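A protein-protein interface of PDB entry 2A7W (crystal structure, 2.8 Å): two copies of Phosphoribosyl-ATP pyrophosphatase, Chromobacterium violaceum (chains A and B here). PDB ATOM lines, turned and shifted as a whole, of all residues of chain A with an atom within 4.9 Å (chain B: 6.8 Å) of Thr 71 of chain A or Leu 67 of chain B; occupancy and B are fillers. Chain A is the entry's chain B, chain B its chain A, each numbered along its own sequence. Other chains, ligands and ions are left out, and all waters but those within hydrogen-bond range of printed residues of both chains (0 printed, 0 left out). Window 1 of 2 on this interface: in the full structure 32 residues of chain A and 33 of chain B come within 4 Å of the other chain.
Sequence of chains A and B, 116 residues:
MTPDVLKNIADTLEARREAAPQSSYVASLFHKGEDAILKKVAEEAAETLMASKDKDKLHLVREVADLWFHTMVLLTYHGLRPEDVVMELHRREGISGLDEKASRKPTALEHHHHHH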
ATOM      1  N   VAL A  41      -8.976  -6.705 -22.974  1.00  0.00           N
ATOM      2  CA  VAL A  41      -8.832  -7.983 -22.290  1.00  0.00           C
ATOM      3  C   VAL A  41     -10.158  -8.731 -22.323  1.00  0.00           C
ATOM      4  O   VAL A  41     -10.224  -9.902 -22.713  1.00  0.00           O
ATOM      5  CB  VAL A  41      -8.363  -7.808 -20.819  1.00  0.00           C
ATOM      6  CG1 VAL A  41      -8.333  -9.134 -20.103  1.00  0.00           C
ATOM      7  CG2 VAL A  41      -6.978  -7.214 -20.782  1.00  0.00           C
ATOM      8  N   LEU A  67      -5.290 -12.376 -26.097  1.00  0.00           N
ATOM      9  CA  LEU A  67      -5.691 -12.240 -24.695  1.00  0.00           C
ATOM     10  C   LEU A  67      -4.438 -12.127 -23.844  1.00  0.00           C
ATOM     11  O   LEU A  67      -4.267 -11.158 -23.117  1.00  0.00           O
ATOM     12  CB  LEU A  67      -6.516 -13.448 -24.247  1.00  0.00           C
ATOM     13  CG  LEU A  67      -6.971 -13.514 -22.794  1.00  0.00           C
ATOM     14  CD1 LEU A  67      -7.898 -12.364 -22.512  1.00  0.00           C
ATOM     15  CD2 LEU A  67      -7.681 -14.821 -22.518  1.00  0.00           C
ATOM     16  N   TRP A  68      -3.550 -13.112 -23.955  1.00  0.00           N
ATOM     17  CA  TRP A  68      -2.299 -13.076 -23.197  1.00  0.00           C
ATOM     18  C   TRP A  68      -1.562 -11.786 -23.484  1.00  0.00           C
ATOM     19  O   TRP A  68      -1.067 -11.130 -22.578  1.00  0.00           O
ATOM     20  CB  TRP A  68      -1.388 -14.239 -23.540  1.00  0.00           C
ATOM     21  CG  TRP A  68      -1.831 -15.528 -23.020  1.00  0.00           C
ATOM     22  CD1 TRP A  68      -3.104 -15.903 -22.712  1.00  0.00           C
ATOM     23  CD2 TRP A  68      -1.013 -16.675 -22.824  1.00  0.00           C
ATOM     24  NE1 TRP A  68      -3.128 -17.234 -22.347  1.00  0.00           N
ATOM     25  CE2 TRP A  68      -1.852 -17.727 -22.409  1.00  0.00           C
ATOM     26  CE3 TRP A  68       0.357 -16.917 -22.972  1.00  0.00           C
ATOM     27  CZ2 TRP A  68      -1.375 -19.002 -22.137  1.00  0.00           C
ATOM     28  CZ3 TRP A  68       0.841 -18.198 -22.705  1.00  0.00           C
ATOM     29  CH2 TRP A  68      -0.028 -19.224 -22.290  1.00  0.00           C
ATOM     30  N   PHE A  69      -1.525 -11.392 -24.743  1.00  0.00           N
ATOM     31  CA  PHE A  69      -0.836 -10.165 -25.096  1.00  0.00           C
ATOM     32  C   PHE A  69      -1.382  -8.965 -24.347  1.00  0.00           C
ATOM     33  O   PHE A  69      -0.626  -8.198 -23.781  1.00  0.00           O
ATOM     34  CB  PHE A  69      -0.903  -9.883 -26.602  1.00  0.00           C
ATOM     35  CG  PHE A  69      -0.217  -8.599 -26.999  1.00  0.00           C
ATOM     36  CD1 PHE A  69       1.168  -8.499 -26.972  1.00  0.00           C
ATOM     37  CD2 PHE A  69      -0.950  -7.475 -27.372  1.00  0.00           C
ATOM     38  CE1 PHE A  69       1.809  -7.290 -27.312  1.00  0.00           C
ATOM     39  CE2 PHE A  69      -0.308  -6.267 -27.710  1.00  0.00           C
ATOM     40  CZ  PHE A  69       1.069  -6.181 -27.677  1.00  0.00           C
ATOM     41  N   HIS A  70      -2.695  -8.784 -24.373  1.00  0.00           N
ATOM     42  CA  HIS A  70      -3.288  -7.648 -23.699  1.00  0.00           C
ATOM     43  C   HIS A  70      -3.171  -7.744 -22.183  1.00  0.00           C
ATOM     44  O   HIS A  70      -3.081  -6.728 -21.482  1.00  0.00           O
ATOM     45  CB  HIS A  70      -4.717  -7.434 -24.176  1.00  0.00           C
ATOM     46  CG  HIS A  70      -4.789  -6.832 -25.543  1.00  0.00           C
ATOM     47  ND1 HIS A  70      -4.918  -7.593 -26.686  1.00  0.00           N
ATOM     48  CD2 HIS A  70      -4.673  -5.549 -25.956  1.00  0.00           C
ATOM     49  CE1 HIS A  70      -4.872  -6.802 -27.744  1.00  0.00           C
ATOM     50  NE2 HIS A  70      -4.725  -5.556 -27.330  1.00  0.00           N
ATOM     51  N   THR A  71      -3.097  -8.975 -21.698  1.00  0.00           N
ATOM     52  CA  THR A  71      -2.925  -9.251 -20.286  1.00  0.00           C
ATOM     53  C   THR A  71      -1.537  -8.715 -19.904  1.00  0.00           C
ATOM     54  O   THR A  71      -1.377  -8.060 -18.881  1.00  0.00           O
ATOM     55  CB  THR A  71      -3.073 -10.780 -20.053  1.00  0.00           C
ATOM     56  OG1 THR A  71      -4.293 -11.036 -19.350  1.00  0.00           O
ATOM     57  CG2 THR A  71      -1.916 -11.358 -19.330  1.00  0.00           C
ATOM     58  N   MET A  72      -0.558  -8.943 -20.775  1.00  0.00           N
ATOM     59  CA  MET A  72       0.811  -8.459 -20.570  1.00  0.00           C
ATOM     60  C   MET A  72       0.854  -6.931 -20.666  1.00  0.00           C
ATOM     61  O   MET A  72       1.654  -6.277 -19.997  1.00  0.00           O
ATOM     62  CB  MET A  72       1.766  -9.040 -21.615  1.00  0.00           C
ATOM     63  CG  MET A  72       2.132 -10.488 -21.414  1.00  0.00           C
ATOM     64  SD  MET A  72       3.487 -10.975 -22.509  1.00  0.00           S
ATOM     65  CE  MET A  72       2.971 -12.595 -22.750  1.00  0.00           C
ATOM     66  N   VAL A  73       0.016  -6.363 -21.521  1.00  0.00           N
ATOM     67  CA  VAL A  73      -0.033  -4.924 -21.651  1.00  0.00           C
ATOM     68  C   VAL A  73      -0.551  -4.380 -20.320  1.00  0.00           C
ATOM     69  O   VAL A  73      -0.050  -3.372 -19.806  1.00  0.00           O
ATOM     70  CB  VAL A  73      -0.994  -4.506 -22.785  1.00  0.00           C
ATOM     71  CG1 VAL A  73      -1.194  -2.988 -22.806  1.00  0.00           C
ATOM     72  CG2 VAL A  73      -0.454  -4.991 -24.104  1.00  0.00           C
ATOM     73  N   LEU A  74      -1.533  -5.080 -19.752  1.00  0.00           N
ATOM     74  CA  LEU A  74      -2.121  -4.682 -18.477  1.00  0.00           C
ATOM     75  C   LEU A  74      -1.049  -4.728 -17.377  1.00  0.00           C
ATOM     76  O   LEU A  74      -0.829  -3.740 -16.682  1.00  0.00           O
ATOM     77  CB  LEU A  74      -3.298  -5.598 -18.125  1.00  0.00           C
ATOM     78  CG  LEU A  74      -4.044  -5.271 -16.844  1.00  0.00           C
ATOM     79  CD1 LEU A  74      -4.764  -3.954 -17.004  1.00  0.00           C
ATOM     80  CD2 LEU A  74      -4.987  -6.386 -16.515  1.00  0.00           C
ATOM     81  N   LEU A  75      -0.379  -5.868 -17.246  1.00  0.00           N
ATOM     82  CA  LEU A  75       0.684  -6.019 -16.263  1.00  0.00           C
ATOM     83  C   LEU A  75       1.703  -4.879 -16.365  1.00  0.00           C
ATOM     84  O   LEU A  75       2.088  -4.273 -15.354  1.00  0.00           O
ATOM     85  CB  LEU A  75       1.407  -7.346 -16.448  1.00  0.00           C
ATOM     86  CG  LEU A  75       0.603  -8.581 -16.098  1.00  0.00           C
ATOM     87  CD1 LEU A  75       1.402  -9.798 -16.451  1.00  0.00           C
ATOM     88  CD2 LEU A  75       0.260  -8.576 -14.628  1.00  0.00           C
ATOM     89  N   LYS B  40     -14.788 -20.834 -16.158  1.00  0.00           N
ATOM     90  CA  LYS B  40     -13.604 -20.458 -15.417  1.00  0.00           C
ATOM     91  C   LYS B  40     -12.782 -19.396 -16.146  1.00  0.00           C
ATOM     92  O   LYS B  40     -12.291 -18.454 -15.527  1.00  0.00           O
ATOM     93  CB  LYS B  40     -12.750 -21.691 -15.137  1.00  0.00           C
ATOM     94  CG  LYS B  40     -12.087 -21.663 -13.772  1.00  0.00           C
ATOM     95  CD  LYS B  40     -13.082 -21.923 -12.645  1.00  0.00           C
ATOM     96  CE  LYS B  40     -13.759 -23.291 -12.802  1.00  0.00           C
ATOM     97  NZ  LYS B  40     -14.539 -23.685 -11.592  1.00  0.00           N
ATOM     98  N   VAL B  41     -12.642 -19.533 -17.459  1.00  0.00           N
ATOM     99  CA  VAL B  41     -11.875 -18.562 -18.218  1.00  0.00           C
ATOM    100  C   VAL B  41     -12.499 -17.183 -18.051  1.00  0.00           C
ATOM    101  O   VAL B  41     -11.810 -16.209 -17.733  1.00  0.00           O
ATOM    102  CB  VAL B  41     -11.816 -18.950 -19.718  1.00  0.00           C
ATOM    103  CG1 VAL B  41     -11.195 -17.830 -20.556  1.00  0.00           C
ATOM    104  CG2 VAL B  41     -11.006 -20.229 -19.868  1.00  0.00           C
ATOM    105  N   ALA B  42     -13.816 -17.127 -18.230  1.00  0.00           N
ATOM    106  CA  ALA B  42     -14.577 -15.891 -18.109  1.00  0.00           C
ATOM    107  C   ALA B  42     -14.463 -15.319 -16.700  1.00  0.00           C
ATOM    108  O   ALA B  42     -14.293 -14.101 -16.524  1.00  0.00           O
ATOM    109  CB  ALA B  42     -16.017 -16.155 -18.442  1.00  0.00           C
ATOM    110  N   GLU B  43     -14.553 -16.212 -15.710  1.00  0.00           N
ATOM    111  CA  GLU B  43     -14.450 -15.842 -14.305  1.00  0.00           C
ATOM    112  C   GLU B  43     -13.136 -15.136 -14.011  1.00  0.00           C
ATOM    113  O   GLU B  43     -13.127 -14.013 -13.496  1.00  0.00           O
ATOM    114  CB  GLU B  43     -14.554 -17.087 -13.436  1.00  0.00           C
ATOM    115  CG  GLU B  43     -14.518 -16.825 -11.938  1.00  0.00           C
ATOM    116  CD  GLU B  43     -14.627 -18.106 -11.124  1.00  0.00           C
ATOM    117  OE1 GLU B  43     -15.562 -18.907 -11.386  1.00  0.00           O
ATOM    118  OE2 GLU B  43     -13.763 -18.308 -10.232  1.00  0.00           O
ATOM    119  N   GLU B  44     -12.032 -15.788 -14.369  1.00  0.00           N
ATOM    120  CA  GLU B  44     -10.710 -15.233 -14.140  1.00  0.00           C
ATOM    121  C   GLU B  44     -10.488 -13.953 -14.920  1.00  0.00           C
ATOM    122  O   GLU B  44      -9.739 -13.084 -14.490  1.00  0.00           O
ATOM    123  CB  GLU B  44      -9.632 -16.254 -14.480  1.00  0.00           C
ATOM    124  CG  GLU B  44      -9.800 -17.585 -13.760  1.00  0.00           C
ATOM    125  CD  GLU B  44      -9.987 -17.423 -12.261  1.00  0.00           C
ATOM    126  OE1 GLU B  44      -9.298 -16.566 -11.668  1.00  0.00           O
ATOM    127  OE2 GLU B  44     -10.817 -18.155 -11.667  1.00  0.00           O
ATOM    128  N   ALA B  45     -11.144 -13.829 -16.064  1.00  0.00           N
ATOM    129  CA  ALA B  45     -11.004 -12.626 -16.878  1.00  0.00           C
ATOM    130  C   ALA B  45     -11.651 -11.458 -16.147  1.00  0.00           C
ATOM    131  O   ALA B  45     -11.094 -10.355 -16.102  1.00  0.00           O
ATOM    132  CB  ALA B  45     -11.673 -12.826 -18.238  1.00  0.00           C
ATOM    133  N   ALA B  46     -12.820 -11.721 -15.558  1.00  0.00           N
ATOM    134  CA  ALA B  46     -13.576 -10.717 -14.821  1.00  0.00           C
ATOM    135  C   ALA B  46     -12.818 -10.289 -13.578  1.00  0.00           C
ATOM    136  O   ALA B  46     -12.732  -9.094 -13.263  1.00  0.00           O
ATOM    137  CB  ALA B  46     -14.920 -11.281 -14.428  1.00  0.00           C
ATOM    138  N   THR B  48      -9.707 -10.384 -13.203  1.00  0.00           N
ATOM    139  CA  THR B  48      -8.539  -9.645 -13.631  1.00  0.00           C
ATOM    140  C   THR B  48      -8.931  -8.181 -13.753  1.00  0.00           C
ATOM    141  O   THR B  48      -8.177  -7.287 -13.366  1.00  0.00           O
ATOM    142  CB  THR B  48      -8.003 -10.184 -14.968  1.00  0.00           C
ATOM    143  OG1 THR B  48      -7.470 -11.497 -14.768  1.00  0.00           O
ATOM    144  CG2 THR B  48      -6.898  -9.294 -15.509  1.00  0.00           C
ATOM    145  N   LEU B  60      -3.909  -9.257  -8.878  1.00  0.00           N
ATOM    146  CA  LEU B  60      -3.855  -9.157 -10.330  1.00  0.00           C
ATOM    147  C   LEU B  60      -3.032 -10.285 -10.927  1.00  0.00           C
ATOM    148  O   LEU B  60      -3.505 -11.030 -11.782  1.00  0.00           O
ATOM    149  CB  LEU B  60      -3.236  -7.826 -10.726  1.00  0.00           C
ATOM    150  CG  LEU B  60      -3.093  -7.583 -12.217  1.00  0.00           C
ATOM    151  CD1 LEU B  60      -4.447  -7.675 -12.903  1.00  0.00           C
ATOM    152  CD2 LEU B  60      -2.510  -6.220 -12.413  1.00  0.00           C
ATOM    153  N   ARG B  62      -2.115 -13.027  -9.497  1.00  0.00           N
ATOM    154  CA  ARG B  62      -2.680 -14.341  -9.193  1.00  0.00           C
ATOM    155  C   ARG B  62      -3.787 -14.707 -10.166  1.00  0.00           C
ATOM    156  O   ARG B  62      -3.891 -15.848 -10.595  1.00  0.00           O
ATOM    157  CB  ARG B  62      -3.223 -14.395  -7.762  1.00  0.00           C
ATOM    158  CG  ARG B  62      -2.196 -14.084  -6.681  1.00  0.00           C
ATOM    159  CD  ARG B  62      -2.372 -14.974  -5.454  1.00  0.00           C
ATOM    160  NE  ARG B  62      -1.900 -16.332  -5.704  1.00  0.00           N
ATOM    161  CZ  ARG B  62      -2.325 -17.411  -5.051  1.00  0.00           C
ATOM    162  NH1 ARG B  62      -3.241 -17.301  -4.096  1.00  0.00           N
ATOM    163  NH2 ARG B  62      -1.823 -18.605  -5.348  1.00  0.00           N
ATOM    164  N   GLU B  63      -4.596 -13.719 -10.527  1.00  0.00           N
ATOM    165  CA  GLU B  63      -5.708 -13.936 -11.442  1.00  0.00           C
ATOM    166  C   GLU B  63      -5.242 -14.108 -12.877  1.00  0.00           C
ATOM    167  O   GLU B  63      -5.684 -15.028 -13.566  1.00  0.00           O
ATOM    168  CB  GLU B  63      -6.737 -12.801 -11.336  1.00  0.00           C
ATOM    169  CG  GLU B  63      -7.404 -12.703  -9.972  1.00  0.00           C
ATOM    170  CD  GLU B  63      -7.986 -14.033  -9.494  1.00  0.00           C
ATOM    171  OE1 GLU B  63      -8.912 -14.555 -10.142  1.00  0.00           O
ATOM    172  OE2 GLU B  63      -7.533 -14.559  -8.454  1.00  0.00           O
ATOM    173  N   VAL B  64      -4.370 -13.215 -13.336  1.00  0.00           N
ATOM    174  CA  VAL B  64      -3.835 -13.328 -14.680  1.00  0.00           C
ATOM    175  C   VAL B  64      -3.213 -14.723 -14.859  1.00  0.00           C
ATOM    176  O   VAL B  64      -3.337 -15.342 -15.906  1.00  0.00           O
ATOM    177  CB  VAL B  64      -2.797 -12.241 -14.962  1.00  0.00           C
ATOM    178  CG1 VAL B  64      -2.018 -12.581 -16.195  1.00  0.00           C
ATOM    179  CG2 VAL B  64      -3.483 -10.905 -15.164  1.00  0.00           C
ATOM    180  N   ALA B  65      -2.597 -15.242 -13.813  1.00  0.00           N
ATOM    181  CA  ALA B  65      -2.004 -16.561 -13.894  1.00  0.00           C
ATOM    182  C   ALA B  65      -3.092 -17.621 -13.954  1.00  0.00           C
ATOM    183  O   ALA B  65      -2.983 -18.600 -14.703  1.00  0.00           O
ATOM    184  CB  ALA B  65      -1.096 -16.812 -12.714  1.00  0.00           C
ATOM    185  N   ASP B  66      -4.142 -17.438 -13.158  1.00  0.00           N
ATOM    186  CA  ASP B  66      -5.255 -18.391 -13.145  1.00  0.00           C
ATOM    187  C   ASP B  66      -5.952 -18.393 -14.519  1.00  0.00           C
ATOM    188  O   ASP B  66      -6.413 -19.432 -15.010  1.00  0.00           O
ATOM    189  CB  ASP B  66      -6.230 -18.044 -12.011  1.00  0.00           C
ATOM    190  CG  ASP B  66      -6.871 -19.283 -11.378  1.00  0.00           C
ATOM    191  OD1 ASP B  66      -6.431 -20.421 -11.674  1.00  0.00           O
ATOM    192  OD2 ASP B  66      -7.813 -19.122 -10.565  1.00  0.00           O
ATOM    193  N   LEU B  67      -5.971 -17.215 -15.139  1.00  0.00           N
ATOM    194  CA  LEU B  67      -6.556 -17.018 -16.465  1.00  0.00           C
ATOM    195  C   LEU B  67      -5.734 -17.813 -17.485  1.00  0.00           C
ATOM    196  O   LEU B  67      -6.256 -18.705 -18.164  1.00  0.00           O
ATOM    197  CB  LEU B  67      -6.569 -15.528 -16.828  1.00  0.00           C
ATOM    198  CG  LEU B  67      -7.101 -15.131 -18.201  1.00  0.00           C
ATOM    199  CD1 LEU B  67      -8.551 -15.530 -18.335  1.00  0.00           C
ATOM    200  CD2 LEU B  67      -6.942 -13.636 -18.402  1.00  0.00           C
ATOM    201  N   TRP B  68      -4.440 -17.508 -17.569  1.00  0.00           N
ATOM    202  CA  TRP B  68      -3.555 -18.237 -18.473  1.00  0.00           C
ATOM    203  C   TRP B  68      -3.694 -19.727 -18.212  1.00  0.00           C
ATOM    204  O   TRP B  68      -3.850 -20.501 -19.149  1.00  0.00           O
ATOM    205  CB  TRP B  68      -2.097 -17.845 -18.281  1.00  0.00           C
ATOM    206  CG  TRP B  68      -1.759 -16.501 -18.807  1.00  0.00           C
ATOM    207  CD1 TRP B  68      -2.602 -15.444 -18.971  1.00  0.00           C
ATOM    208  CD2 TRP B  68      -0.455 -16.035 -19.160  1.00  0.00           C
ATOM    209  NE1 TRP B  68      -1.899 -14.343 -19.394  1.00  0.00           N
ATOM    210  CE2 TRP B  68      -0.577 -14.681 -19.518  1.00  0.00           C
ATOM    211  CE3 TRP B  68       0.811 -16.638 -19.198  1.00  0.00           C
ATOM    212  CZ2 TRP B  68       0.516 -13.906 -19.906  1.00  0.00           C
ATOM    213  CZ3 TRP B  68       1.907 -15.869 -19.583  1.00  0.00           C
ATOM    214  CH2 TRP B  68       1.746 -14.513 -19.934  1.00  0.00           C
ATOM    215  N   PHE B  69      -3.696 -20.125 -16.941  1.00  0.00           N
ATOM    216  CA  PHE B  69      -3.809 -21.534 -16.615  1.00  0.00           C
ATOM    217  C   PHE B  69      -5.037 -22.179 -17.220  1.00  0.00           C
ATOM    218  O   PHE B  69      -4.953 -23.239 -17.838  1.00  0.00           O
ATOM    219  CB  PHE B  69      -3.826 -21.766 -15.105  1.00  0.00           C
ATOM    220  CG  PHE B  69      -3.937 -23.223 -14.730  1.00  0.00           C
ATOM    221  CD1 PHE B  69      -2.854 -24.085 -14.909  1.00  0.00           C
ATOM    222  CD2 PHE B  69      -5.143 -23.748 -14.270  1.00  0.00           C
ATOM    223  CE1 PHE B  69      -2.972 -25.453 -14.641  1.00  0.00           C
ATOM    224  CE2 PHE B  69      -5.274 -25.115 -13.997  1.00  0.00           C
ATOM    225  CZ  PHE B  69      -4.183 -25.970 -14.186  1.00  0.00           C
ATOM    226  N   HIS B  70      -6.190 -21.556 -17.018  1.00  0.00           N
ATOM    227  CA  HIS B  70      -7.417 -22.123 -17.561  1.00  0.00           C
ATOM    228  C   HIS B  70      -7.480 -22.027 -19.084  1.00  0.00           C
ATOM    229  O   HIS B  70      -8.142 -22.834 -19.748  1.00  0.00           O
ATOM    230  CB  HIS B  70      -8.627 -21.508 -16.879  1.00  0.00           C
ATOM    231  CG  HIS B  70      -8.808 -21.997 -15.481  1.00  0.00           C
ATOM    232  ND1 HIS B  70      -8.269 -21.351 -14.387  1.00  0.00           N
ATOM    233  CD2 HIS B  70      -9.421 -23.106 -15.002  1.00  0.00           C
ATOM    234  CE1 HIS B  70      -8.543 -22.042 -13.296  1.00  0.00           C
ATOM    235  NE2 HIS B  70      -9.242 -23.112 -13.639  1.00  0.00           N
ATOM    236  N   THR B  71      -6.742 -21.065 -19.624  1.00  0.00           N
ATOM    237  CA  THR B  71      -6.656 -20.870 -21.053  1.00  0.00           C
ATOM    238  C   THR B  71      -5.920 -22.106 -21.613  1.00  0.00           C
ATOM    239  O   THR B  71      -6.333 -22.693 -22.622  1.00  0.00           O
ATOM    240  CB  THR B  71      -5.911 -19.549 -21.314  1.00  0.00           C
ATOM    241  OG1 THR B  71      -6.839 -18.585 -21.804  1.00  0.00           O
ATOM    242  CG2 THR B  71      -4.776 -19.704 -22.265  1.00  0.00           C
ATOM    243  N   MET B  72      -4.883 -22.534 -20.891  1.00  0.00           N
ATOM    244  CA  MET B  72      -4.094 -23.706 -21.256  1.00  0.00           C
ATOM    245  C   MET B  72      -4.941 -24.966 -21.120  1.00  0.00           C
ATOM    246  O   MET B  72      -4.787 -25.921 -21.877  1.00  0.00           O
ATOM    247  CB  MET B  72      -2.850 -23.825 -20.371  1.00  0.00           C
ATOM    248  CG  MET B  72      -1.744 -22.849 -20.692  1.00  0.00           C
ATOM    249  SD  MET B  72      -0.292 -23.123 -19.660  1.00  0.00           S
ATOM    250  CE  MET B  72       0.315 -21.489 -19.606  1.00  0.00           C
ATOM    251  N   VAL B  73      -5.825 -24.972 -20.136  1.00  0.00           N
ATOM    252  CA  VAL B  73      -6.697 -26.113 -19.937  1.00  0.00           C
ATOM    253  C   VAL B  73      -7.621 -26.202 -21.137  1.00  0.00           C
ATOM    254  O   VAL B  73      -7.924 -27.290 -21.632  1.00  0.00           O
ATOM    255  CB  VAL B  73      -7.544 -25.952 -18.671  1.00  0.00           C
ATOM    256  CG1 VAL B  73      -8.595 -27.058 -18.593  1.00  0.00           C
ATOM    257  CG2 VAL B  73      -6.641 -25.950 -17.445  1.00  0.00           C
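OG1 of Thr 48 of chain B lies within hydrogen-bond range of O of Glu 44 of chain B (2.8 Å).
Leu 67 of chain A touches Thr 71 of chain B (CD2 to OG1, 3.9 Å). Trp 68 of chain A touches Trp 68 of chain B (CD2 to CD2, 3.8 Å). Trp 68 of chain A touches Thr 71 of chain B (NE1 to CG2, 3.0 Å). Trp 68 of chain A touches Met 72 of chain B. Val 64 of chain B touches Thr 71 of chain A. CD2 of Leu 67 of chain B touches OG1 of Thr 71 of chain A, at 3.8 Å. CG2 of Thr 71 of chain A touches NE1 of Trp 68 of chain B, 3.0 Å away. CH2 of Trp 68 of chain B touches CE of Met 72 of chain A (3.6 Å). Leu 74 of chain A touches Thr 48 of chain B. Leu 74 of chain A touches Leu 60 of chain B (CD2 to CD1, 3.9 Å).
Thr 71 of chain A touches three residues of chain B. Printed residues of chain B within 4 Å of Met 72 of chain A: Trp 68 (3.6 Å). Printed residues of chain A within 4 Å of Thr 48 of chain B: Leu 74. Of the printed residues of chain A, Leu 60 of chain B touches Leu 74. Printed residues of chain A within 4 Å of Val 64 of chain B: Thr 71 (3.4 Å). Printed residues of chain A within 4 Å of Trp 68 of chain B: Trp 68 (3.8 Å), Thr 71 (3.0 Å) and Met 72 (3.6 Å). The nearest printed residue of chain A that does not touch Leu 60 of chain B is Leu 75 of chain A (4.2 Å).
Of the 10 printed residues of chain A, 5 touch a printed residue of chain B. Hydrophobic or aromatic side chains of chain A that line the printed part of chain B: Leu 67, Trp 68, Met 72 and Leu 74. Hydrophobic or aromatic side chains of chain B that line the printed part of chain A: Leu 60, Val 64, Leu 67, Trp 68 and Met 72.
Leu 67 of chain A touches Thr 71 of chain B, and with the chains exchanged Thr 71 of chain A touches Leu 67 of chain B. Trp 68 of chain A touches its own counterpart, Trp 68 of chain B. Trp 68 of chain A touches Thr 71 of chain B, and with the chains exchanged Thr 71 of chain A touches Trp 68 of chain B. Trp 68 of chain A touches Met 72 of chain B, and with the chains exchanged Met 72 of chain A touches Trp 68 of chain B. Of the 10 pairs that touch across the chains among the printed residues, 7 have their exchanged pair printed and touching as well.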
